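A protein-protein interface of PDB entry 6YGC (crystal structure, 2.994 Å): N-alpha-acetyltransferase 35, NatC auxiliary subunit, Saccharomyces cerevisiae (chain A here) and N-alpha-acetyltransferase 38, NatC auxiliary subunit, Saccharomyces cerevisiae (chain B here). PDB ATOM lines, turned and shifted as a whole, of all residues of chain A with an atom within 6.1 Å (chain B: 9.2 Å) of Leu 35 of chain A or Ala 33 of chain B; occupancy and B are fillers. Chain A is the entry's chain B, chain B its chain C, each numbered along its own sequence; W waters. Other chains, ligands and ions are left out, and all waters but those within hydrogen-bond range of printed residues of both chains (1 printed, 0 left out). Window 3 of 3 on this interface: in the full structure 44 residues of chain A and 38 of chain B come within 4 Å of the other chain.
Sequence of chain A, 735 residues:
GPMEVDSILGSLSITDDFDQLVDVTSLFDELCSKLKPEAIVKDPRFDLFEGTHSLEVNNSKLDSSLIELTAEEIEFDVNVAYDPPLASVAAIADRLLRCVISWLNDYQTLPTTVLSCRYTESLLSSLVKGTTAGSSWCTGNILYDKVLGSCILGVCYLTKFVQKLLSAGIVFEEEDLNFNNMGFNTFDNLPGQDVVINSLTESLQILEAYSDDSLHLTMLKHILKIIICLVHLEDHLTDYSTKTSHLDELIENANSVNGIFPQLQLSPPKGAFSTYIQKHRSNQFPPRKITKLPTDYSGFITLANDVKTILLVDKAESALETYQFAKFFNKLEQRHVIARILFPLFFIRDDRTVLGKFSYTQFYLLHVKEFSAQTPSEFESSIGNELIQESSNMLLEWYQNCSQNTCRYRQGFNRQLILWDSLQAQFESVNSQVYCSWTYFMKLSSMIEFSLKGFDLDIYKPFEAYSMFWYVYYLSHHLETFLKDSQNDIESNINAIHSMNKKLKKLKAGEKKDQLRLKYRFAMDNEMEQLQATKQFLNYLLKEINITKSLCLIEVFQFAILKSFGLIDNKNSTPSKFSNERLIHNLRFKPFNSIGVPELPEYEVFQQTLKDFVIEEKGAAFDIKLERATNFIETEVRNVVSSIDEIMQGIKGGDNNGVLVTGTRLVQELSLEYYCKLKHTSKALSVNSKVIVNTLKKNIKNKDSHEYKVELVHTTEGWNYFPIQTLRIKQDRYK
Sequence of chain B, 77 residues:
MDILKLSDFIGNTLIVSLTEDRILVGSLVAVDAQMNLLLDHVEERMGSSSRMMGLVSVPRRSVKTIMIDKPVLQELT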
ATOM      1  N   GLU A  30      18.354 -30.879   5.800  1.00  0.00           N
ATOM      2  CA  GLU A  30      19.578 -30.126   6.051  1.00  0.00           C
ATOM      3  C   GLU A  30      19.424 -28.656   5.680  1.00  0.00           C
ATOM      4  O   GLU A  30      20.047 -27.793   6.309  1.00  0.00           O
ATOM      5  CB  GLU A  30      20.746 -30.754   5.291  1.00  0.00           C
ATOM      6  CG  GLU A  30      20.994 -32.210   5.649  1.00  0.00           C
ATOM      7  CD  GLU A  30      22.321 -32.721   5.133  1.00  0.00           C
ATOM      8  OE1 GLU A  30      23.161 -31.893   4.726  1.00  0.00           O
ATOM      9  OE2 GLU A  30      22.527 -33.953   5.136  1.00  0.00           O
ATOM     10  N   LEU A  31      18.606 -28.349   4.671  1.00  0.00           N
ATOM     11  CA  LEU A  31      18.390 -26.953   4.308  1.00  0.00           C
ATOM     12  C   LEU A  31      17.531 -26.239   5.345  1.00  0.00           C
ATOM     13  O   LEU A  31      17.816 -25.092   5.709  1.00  0.00           O
ATOM     14  CB  LEU A  31      17.751 -26.856   2.924  1.00  0.00           C
ATOM     15  CG  LEU A  31      18.710 -26.569   1.767  1.00  0.00           C
ATOM     16  CD1 LEU A  31      17.925 -26.210   0.523  1.00  0.00           C
ATOM     17  CD2 LEU A  31      19.678 -25.456   2.134  1.00  0.00           C
ATOM     18  N   CYS A  32      16.469 -26.893   5.822  1.00  0.00           N
ATOM     19  CA  CYS A  32      15.663 -26.302   6.885  1.00  0.00           C
ATOM     20  C   CYS A  32      16.440 -26.221   8.191  1.00  0.00           C
ATOM     21  O   CYS A  32      16.237 -25.289   8.977  1.00  0.00           O
ATOM     22  CB  CYS A  32      14.376 -27.101   7.078  1.00  0.00           C
ATOM     23  SG  CYS A  32      13.259 -27.045   5.660  1.00  0.00           S
ATOM     24  N   SER A  33      17.329 -27.185   8.440  1.00  0.00           N
ATOM     25  CA  SER A  33      18.241 -27.088   9.572  1.00  0.00           C
ATOM     26  C   SER A  33      19.206 -25.920   9.423  1.00  0.00           C
ATOM     27  O   SER A  33      19.736 -25.431  10.426  1.00  0.00           O
ATOM     28  CB  SER A  33      19.020 -28.395   9.732  1.00  0.00           C
ATOM     29  OG  SER A  33      20.169 -28.217  10.542  1.00  0.00           O
ATOM     30  N   LYS A  34      19.442 -25.465   8.192  1.00  0.00           N
ATOM     31  CA  LYS A  34      20.352 -24.351   7.951  1.00  0.00           C
ATOM     32  C   LYS A  34      19.688 -23.003   8.210  1.00  0.00           C
ATOM     33  O   LYS A  34      20.376 -22.028   8.529  1.00  0.00           O
ATOM     34  CB  LYS A  34      20.877 -24.430   6.514  1.00  0.00           C
ATOM     35  CG  LYS A  34      21.862 -23.348   6.111  1.00  0.00           C
ATOM     36  CD  LYS A  34      22.232 -23.496   4.645  1.00  0.00           C
ATOM     37  CE  LYS A  34      23.055 -22.321   4.151  1.00  0.00           C
ATOM     38  NZ  LYS A  34      23.333 -22.419   2.691  1.00  0.00           N
ATOM     39  N   LEU A  35      18.363 -22.934   8.093  1.00  0.00           N
ATOM     40  CA  LEU A  35      17.655 -21.675   8.268  1.00  0.00           C
ATOM     41  C   LEU A  35      17.646 -21.245   9.730  1.00  0.00           C
ATOM     42  O   LEU A  35      17.718 -22.069  10.647  1.00  0.00           O
ATOM     43  CB  LEU A  35      16.216 -21.798   7.763  1.00  0.00           C
ATOM     44  CG  LEU A  35      16.001 -22.109   6.282  1.00  0.00           C
ATOM     45  CD1 LEU A  35      14.526 -22.351   6.012  1.00  0.00           C
ATOM     46  CD2 LEU A  35      16.531 -20.983   5.408  1.00  0.00           C
ATOM     47  N   LYS A  36      17.560 -19.935   9.939  1.00  0.00           N
ATOM     48  CA  LYS A  36      17.378 -19.406  11.278  1.00  0.00           C
ATOM     49  C   LYS A  36      15.976 -19.748  11.783  1.00  0.00           C
ATOM     50  O   LYS A  36      15.028 -19.825  10.998  1.00  0.00           O
ATOM     51  CB  LYS A  36      17.584 -17.894  11.291  1.00  0.00           C
ATOM     52  CG  LYS A  36      19.005 -17.455  10.975  1.00  0.00           C
ATOM     53  CD  LYS A  36      19.172 -15.955  11.169  1.00  0.00           C
ATOM     54  CE  LYS A  36      20.607 -15.518  10.916  1.00  0.00           C
ATOM     55  NZ  LYS A  36      20.796 -14.062  11.169  1.00  0.00           N
ATOM     56  N   PRO A  37      15.819 -19.955  13.095  1.00  0.00           N
ATOM     57  CA  PRO A  37      14.512 -20.394  13.612  1.00  0.00           C
ATOM     58  C   PRO A  37      13.378 -19.420  13.336  1.00  0.00           C
ATOM     59  O   PRO A  37      12.230 -19.853  13.180  1.00  0.00           O
ATOM     60  CB  PRO A  37      14.767 -20.551  15.119  1.00  0.00           C
ATOM     61  CG  PRO A  37      15.975 -19.712  15.396  1.00  0.00           C
ATOM     62  CD  PRO A  37      16.819 -19.813  14.166  1.00  0.00           C
ATOM     63  N   GLU A  38      13.660 -18.120  13.256  1.00  0.00           N
ATOM     64  CA  GLU A  38      12.599 -17.141  13.059  1.00  0.00           C
ATOM     65  C   GLU A  38      12.158 -17.027  11.606  1.00  0.00           C
ATOM     66  O   GLU A  38      11.030 -16.593  11.347  1.00  0.00           O
ATOM     67  CB  GLU A  38      13.043 -15.768  13.567  1.00  0.00           C
ATOM     68  CG  GLU A  38      14.259 -15.191  12.855  1.00  0.00           C
ATOM     69  CD  GLU A  38      15.555 -15.444  13.603  1.00  0.00           C
ATOM     70  OE1 GLU A  38      15.617 -16.422  14.378  1.00  0.00           O
ATOM     71  OE2 GLU A  38      16.507 -14.657  13.422  1.00  0.00           O
ATOM     72  N   ALA A  39      13.009 -17.411  10.659  1.00  0.00           N
ATOM     73  CA  ALA A  39      12.734 -17.166   9.252  1.00  0.00           C
ATOM     74  C   ALA A  39      11.724 -18.162   8.694  1.00  0.00           C
ATOM     75  O   ALA A  39      11.631 -19.309   9.141  1.00  0.00           O
ATOM     76  CB  ALA A  39      14.024 -17.229   8.435  1.00  0.00           C
ATOM     77  N   ILE A  40      10.965 -17.705   7.699  1.00  0.00           N
ATOM     78  CA  ILE A  40      10.019 -18.536   6.961  1.00  0.00           C
ATOM     79  C   ILE A  40      10.273 -18.319   5.478  1.00  0.00           C
ATOM     80  O   ILE A  40      10.199 -17.185   4.992  1.00  0.00           O
ATOM     81  CB  ILE A  40       8.558 -18.205   7.306  1.00  0.00           C
ATOM     82  CG1 ILE A  40       8.283 -18.440   8.792  1.00  0.00           C
ATOM     83  CG2 ILE A  40       7.611 -19.031   6.447  1.00  0.00           C
ATOM     84  CD1 ILE A  40       6.860 -18.131   9.196  1.00  0.00           C
ATOM     85  N   VAL A  41      10.576 -19.397   4.762  1.00  0.00           N
ATOM     86  CA  VAL A  41      10.780 -19.320   3.319  1.00  0.00           C
ATOM     87  C   VAL A  41       9.425 -19.346   2.631  1.00  0.00           C
ATOM     88  O   VAL A  41       8.618 -20.255   2.859  1.00  0.00           O
ATOM     89  CB  VAL A  41      11.672 -20.471   2.831  1.00  0.00           C
ATOM     90  CG1 VAL A  41      11.543 -20.633   1.325  1.00  0.00           C
ATOM     91  CG2 VAL A  41      13.117 -20.216   3.217  1.00  0.00           C
ATOM     92  N   LYS B   5      18.685 -23.490  -3.460  1.00  0.00           N
ATOM     93  CA  LYS B   5      18.059 -22.812  -2.337  1.00  0.00           C
ATOM     94  C   LYS B   5      16.604 -23.247  -2.204  1.00  0.00           C
ATOM     95  O   LYS B   5      15.971 -23.674  -3.172  1.00  0.00           O
ATOM     96  CB  LYS B   5      18.139 -21.295  -2.510  1.00  0.00           C
ATOM     97  CG  LYS B   5      19.489 -20.809  -3.006  1.00  0.00           C
ATOM     98  CD  LYS B   5      19.639 -19.307  -2.850  1.00  0.00           C
ATOM     99  CE  LYS B   5      21.005 -18.847  -3.335  1.00  0.00           C
ATOM    100  NZ  LYS B   5      21.500 -17.668  -2.575  1.00  0.00           N
ATOM    101  N   LEU B   6      16.076 -23.140  -0.982  1.00  0.00           N
ATOM    102  CA  LEU B   6      14.684 -23.512  -0.748  1.00  0.00           C
ATOM    103  C   LEU B   6      13.724 -22.602  -1.506  1.00  0.00           C
ATOM    104  O   LEU B   6      12.628 -23.032  -1.882  1.00  0.00           O
ATOM    105  CB  LEU B   6      14.371 -23.482   0.747  1.00  0.00           C
ATOM    106  CG  LEU B   6      14.806 -24.693   1.573  1.00  0.00           C
ATOM    107  CD1 LEU B   6      14.423 -24.505   3.029  1.00  0.00           C
ATOM    108  CD2 LEU B   6      14.193 -25.970   1.017  1.00  0.00           C
ATOM    109  N   SER B   7      14.118 -21.349  -1.743  1.00  0.00           N
ATOM    110  CA  SER B   7      13.275 -20.420  -2.486  1.00  0.00           C
ATOM    111  C   SER B   7      13.003 -20.897  -3.906  1.00  0.00           C
ATOM    112  O   SER B   7      12.018 -20.467  -4.517  1.00  0.00           O
ATOM    113  CB  SER B   7      13.922 -19.036  -2.513  1.00  0.00           C
ATOM    114  OG  SER B   7      15.188 -19.080  -3.150  1.00  0.00           O
ATOM    115  N   ALA B  30       5.045 -22.385   1.605  1.00  0.00           N
ATOM    116  CA  ALA B  30       5.949 -21.889   2.631  1.00  0.00           C
ATOM    117  C   ALA B  30       6.582 -23.057   3.372  1.00  0.00           C
ATOM    118  O   ALA B  30       6.039 -24.164   3.412  1.00  0.00           O
ATOM    119  CB  ALA B  30       5.230 -20.960   3.618  1.00  0.00           C
ATOM    120  N   VAL B  31       7.744 -22.788   3.963  1.00  0.00           N
ATOM    121  CA  VAL B  31       8.459 -23.757   4.788  1.00  0.00           C
ATOM    122  C   VAL B  31       9.284 -22.984   5.810  1.00  0.00           C
ATOM    123  O   VAL B  31       9.848 -21.930   5.501  1.00  0.00           O
ATOM    124  CB  VAL B  31       9.333 -24.700   3.930  1.00  0.00           C
ATOM    125  CG1 VAL B  31      10.382 -23.917   3.151  1.00  0.00           C
ATOM    126  CG2 VAL B  31       9.985 -25.769   4.798  1.00  0.00           C
ATOM    127  N   ASP B  32       9.335 -23.497   7.037  1.00  0.00           N
ATOM    128  CA  ASP B  32       9.997 -22.819   8.141  1.00  0.00           C
ATOM    129  C   ASP B  32      11.274 -23.564   8.529  1.00  0.00           C
ATOM    130  O   ASP B  32      11.686 -24.526   7.871  1.00  0.00           O
ATOM    131  CB  ASP B  32       9.036 -22.675   9.327  1.00  0.00           C
ATOM    132  CG  ASP B  32       8.513 -24.009   9.828  1.00  0.00           C
ATOM    133  OD1 ASP B  32       8.829 -25.049   9.212  1.00  0.00           O
ATOM    134  OD2 ASP B  32       7.783 -24.016  10.841  1.00  0.00           O
ATOM    135  N   ALA B  33      11.903 -23.114   9.618  1.00  0.00           N
ATOM    136  CA  ALA B  33      13.160 -23.719  10.045  1.00  0.00           C
ATOM    137  C   ALA B  33      12.943 -25.080  10.688  1.00  0.00           C
ATOM    138  O   ALA B  33      13.857 -25.912  10.694  1.00  0.00           O
ATOM    139  CB  ALA B  33      13.891 -22.795  11.013  1.00  0.00           C
ATOM    140  N   GLN B  34      11.759 -25.322  11.244  1.00  0.00           N
ATOM    141  CA  GLN B  34      11.424 -26.626  11.799  1.00  0.00           C
ATOM    142  C   GLN B  34      10.925 -27.596  10.734  1.00  0.00           C
ATOM    143  O   GLN B  34      10.500 -28.707  11.073  1.00  0.00           O
ATOM    144  CB  GLN B  34      10.379 -26.469  12.908  1.00  0.00           C
ATOM    145  CG  GLN B  34      10.451 -27.534  13.991  1.00  0.00           C
ATOM    146  CD  GLN B  34       9.484 -27.276  15.129  1.00  0.00           C
ATOM    147  OE1 GLN B  34       8.807 -26.248  15.167  1.00  0.00           O
ATOM    148  NE2 GLN B  34       9.415 -28.213  16.067  1.00  0.00           N
ATOM    149  N   MET B  35      10.972 -27.190   9.465  1.00  0.00           N
ATOM    150  CA  MET B  35      10.553 -28.012   8.328  1.00  0.00           C
ATOM    151  C   MET B  35       9.077 -28.399   8.434  1.00  0.00           C
ATOM    152  O   MET B  35       8.706 -29.571   8.338  1.00  0.00           O
ATOM    153  CB  MET B  35      11.441 -29.251   8.177  1.00  0.00           C
ATOM    154  CG  MET B  35      11.409 -29.861   6.782  1.00  0.00           C
ATOM    155  SD  MET B  35      12.442 -31.328   6.621  1.00  0.00           S
ATOM    156  CE  MET B  35      11.577 -32.474   7.690  1.00  0.00           C
ATOM    157  N   ASN B  36       8.231 -27.394   8.637  1.00  0.00           N
ATOM    158  CA  ASN B  36       6.786 -27.551   8.532  1.00  0.00           C
ATOM    159  C   ASN B  36       6.343 -27.004   7.182  1.00  0.00           C
ATOM    160  O   ASN B  36       6.707 -25.883   6.812  1.00  0.00           O
ATOM    161  CB  ASN B  36       6.065 -26.829   9.671  1.00  0.00           C
ATOM    162  CG  ASN B  36       6.551 -27.265  11.040  1.00  0.00           C
ATOM    163  OD1 ASN B  36       6.298 -28.389  11.474  1.00  0.00           O
ATOM    164  ND2 ASN B  36       7.247 -26.370  11.732  1.00  0.00           N
ATOM    165  N   LEU B  37       5.570 -27.797   6.449  1.00  0.00           N
ATOM    166  CA  LEU B  37       5.232 -27.490   5.067  1.00  0.00           C
ATOM    167  C   LEU B  37       3.825 -26.918   4.966  1.00  0.00           C
ATOM    168  O   LEU B  37       2.910 -27.358   5.668  1.00  0.00           O
ATOM    169  CB  LEU B  37       5.343 -28.740   4.193  1.00  0.00           C
ATOM    170  CG  LEU B  37       6.705 -29.436   4.154  1.00  0.00           C
ATOM    171  CD1 LEU B  37       6.607 -30.734   3.372  1.00  0.00           C
ATOM    172  CD2 LEU B  37       7.762 -28.523   3.554  1.00  0.00           C
ATOM    173  N   ARG B  60       6.454 -31.640  10.587  1.00  0.00           N
ATOM    174  CA  ARG B  60       7.652 -32.415  10.274  1.00  0.00           C
ATOM    175  C   ARG B  60       7.472 -33.890  10.618  1.00  0.00           C
ATOM    176  O   ARG B  60       7.858 -34.765   9.834  1.00  0.00           O
ATOM    177  CB  ARG B  60       8.859 -31.835  11.015  1.00  0.00           C
ATOM    178  CG  ARG B  60      10.088 -32.737  11.012  1.00  0.00           C
ATOM    179  CD  ARG B  60      11.208 -32.151  11.861  1.00  0.00           C
ATOM    180  NE  ARG B  60      12.286 -33.112  12.087  1.00  0.00           N
ATOM    181  CZ  ARG B  60      13.408 -33.162  11.377  1.00  0.00           C
ATOM    182  NH1 ARG B  60      13.610 -32.303  10.387  1.00  0.00           N
ATOM    183  NH2 ARG B  60      14.333 -34.070  11.657  1.00  0.00           N
HETATM  184  O   HOH W   1      15.460 -28.880  10.076  1.00  0.00           O
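The backbone carbonyl oxygen of Ala 33 of chain B sits close to the backbone carbonyl oxygen of Cys 32 of chain A (3.0 Å). N of Val 41 of chain A is in hydrogen-bond range of O of Val 31 of chain B (2.7 Å). The side-chain sulfur of Cys 32 of chain A lies within hydrogen-bond range of the backbone carbonyl oxygen of Asp 32 of chain B, 3.7 Å away.
OD1 of Asp 32 of chain B sits at hydrogen-bond distance from N of Met 35 of chain B. The side-chain carboxylate (OD1) of Asp 32 of chain B lies within hydrogen-bond range of the backbone NH (N) of Asn 36 of chain B, at 2.5 Å.
Among the printed residues, pairs that only touch across the chains: Leu 31 of chain A with Leu 6 of chain B, Cys 32 of chain A with Leu 6 of chain B, Cys 32 of chain A with Val 31 of chain B, Cys 32 of chain A with Met 35 of chain B, Leu 35 of chain A with Leu 6 of chain B, Leu 35 of chain A with Ala 33 of chain B, Lys 36 of chain A with Ala 33 of chain B, Pro 37 of chain A with Ala 33 of chain B, Ala 39 of chain A with Asp 32 of chain B, Ala 39 of chain A with Ala 33 of chain B, Ile 40 of chain A with Val 31 of chain B and Val 41 of chain A with Ala 30 of chain B.
Of chain B, only Leu 6, Val 31, Asp 32, Ala 33 and Met 35 come within 4 Å of Cys 32 of chain A. Leu 35 of chain A touches just these residues of chain B: Leu 6 and Ala 33. Of the printed residues of chain B, Val 41 of chain A touches Ala 30 and Val 31. Of the printed residues of chain A, Leu 6 of chain B touches Leu 31 (3.6 Å), Cys 32 (3.8 Å) and Leu 35 (3.7 Å). Of the printed residues of chain A, Val 31 of chain B touches Cys 32 (3.6 Å), Ile 40 (3.6 Å) and Val 41 (2.7 Å). Of the printed residues of chain A, Met 35 of chain B touches Cys 32 (3.6 Å). The nearest residue of chain B that does not touch Leu 35 of chain A is Asp 32 of chain B (4.03 Å). The nearest residue of chain A that does not touch Ala 33 of chain B is Ser 33 of chain A (4.3 Å).
Of the 12 printed residues of chain B, 6 touch a printed residue of chain A. Hydrophobic or aromatic side chains of chain B within 4 Å of the printed part of chain A: Leu 6, Ala 30, Val 31, Ala 33 and Met 35. Along chain B the printed residues that touch a printed residue of chain A span positions 6 to 35. Among the printed residues, no Asp or Glu carboxylate lies within 4 Å of a Lys or Arg side-chain nitrogen of the other chain.
Water W1 bridges the backbone NH of Ser 33 of chain A and the backbone carbonyl oxygen of Ala 33 of chain B.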
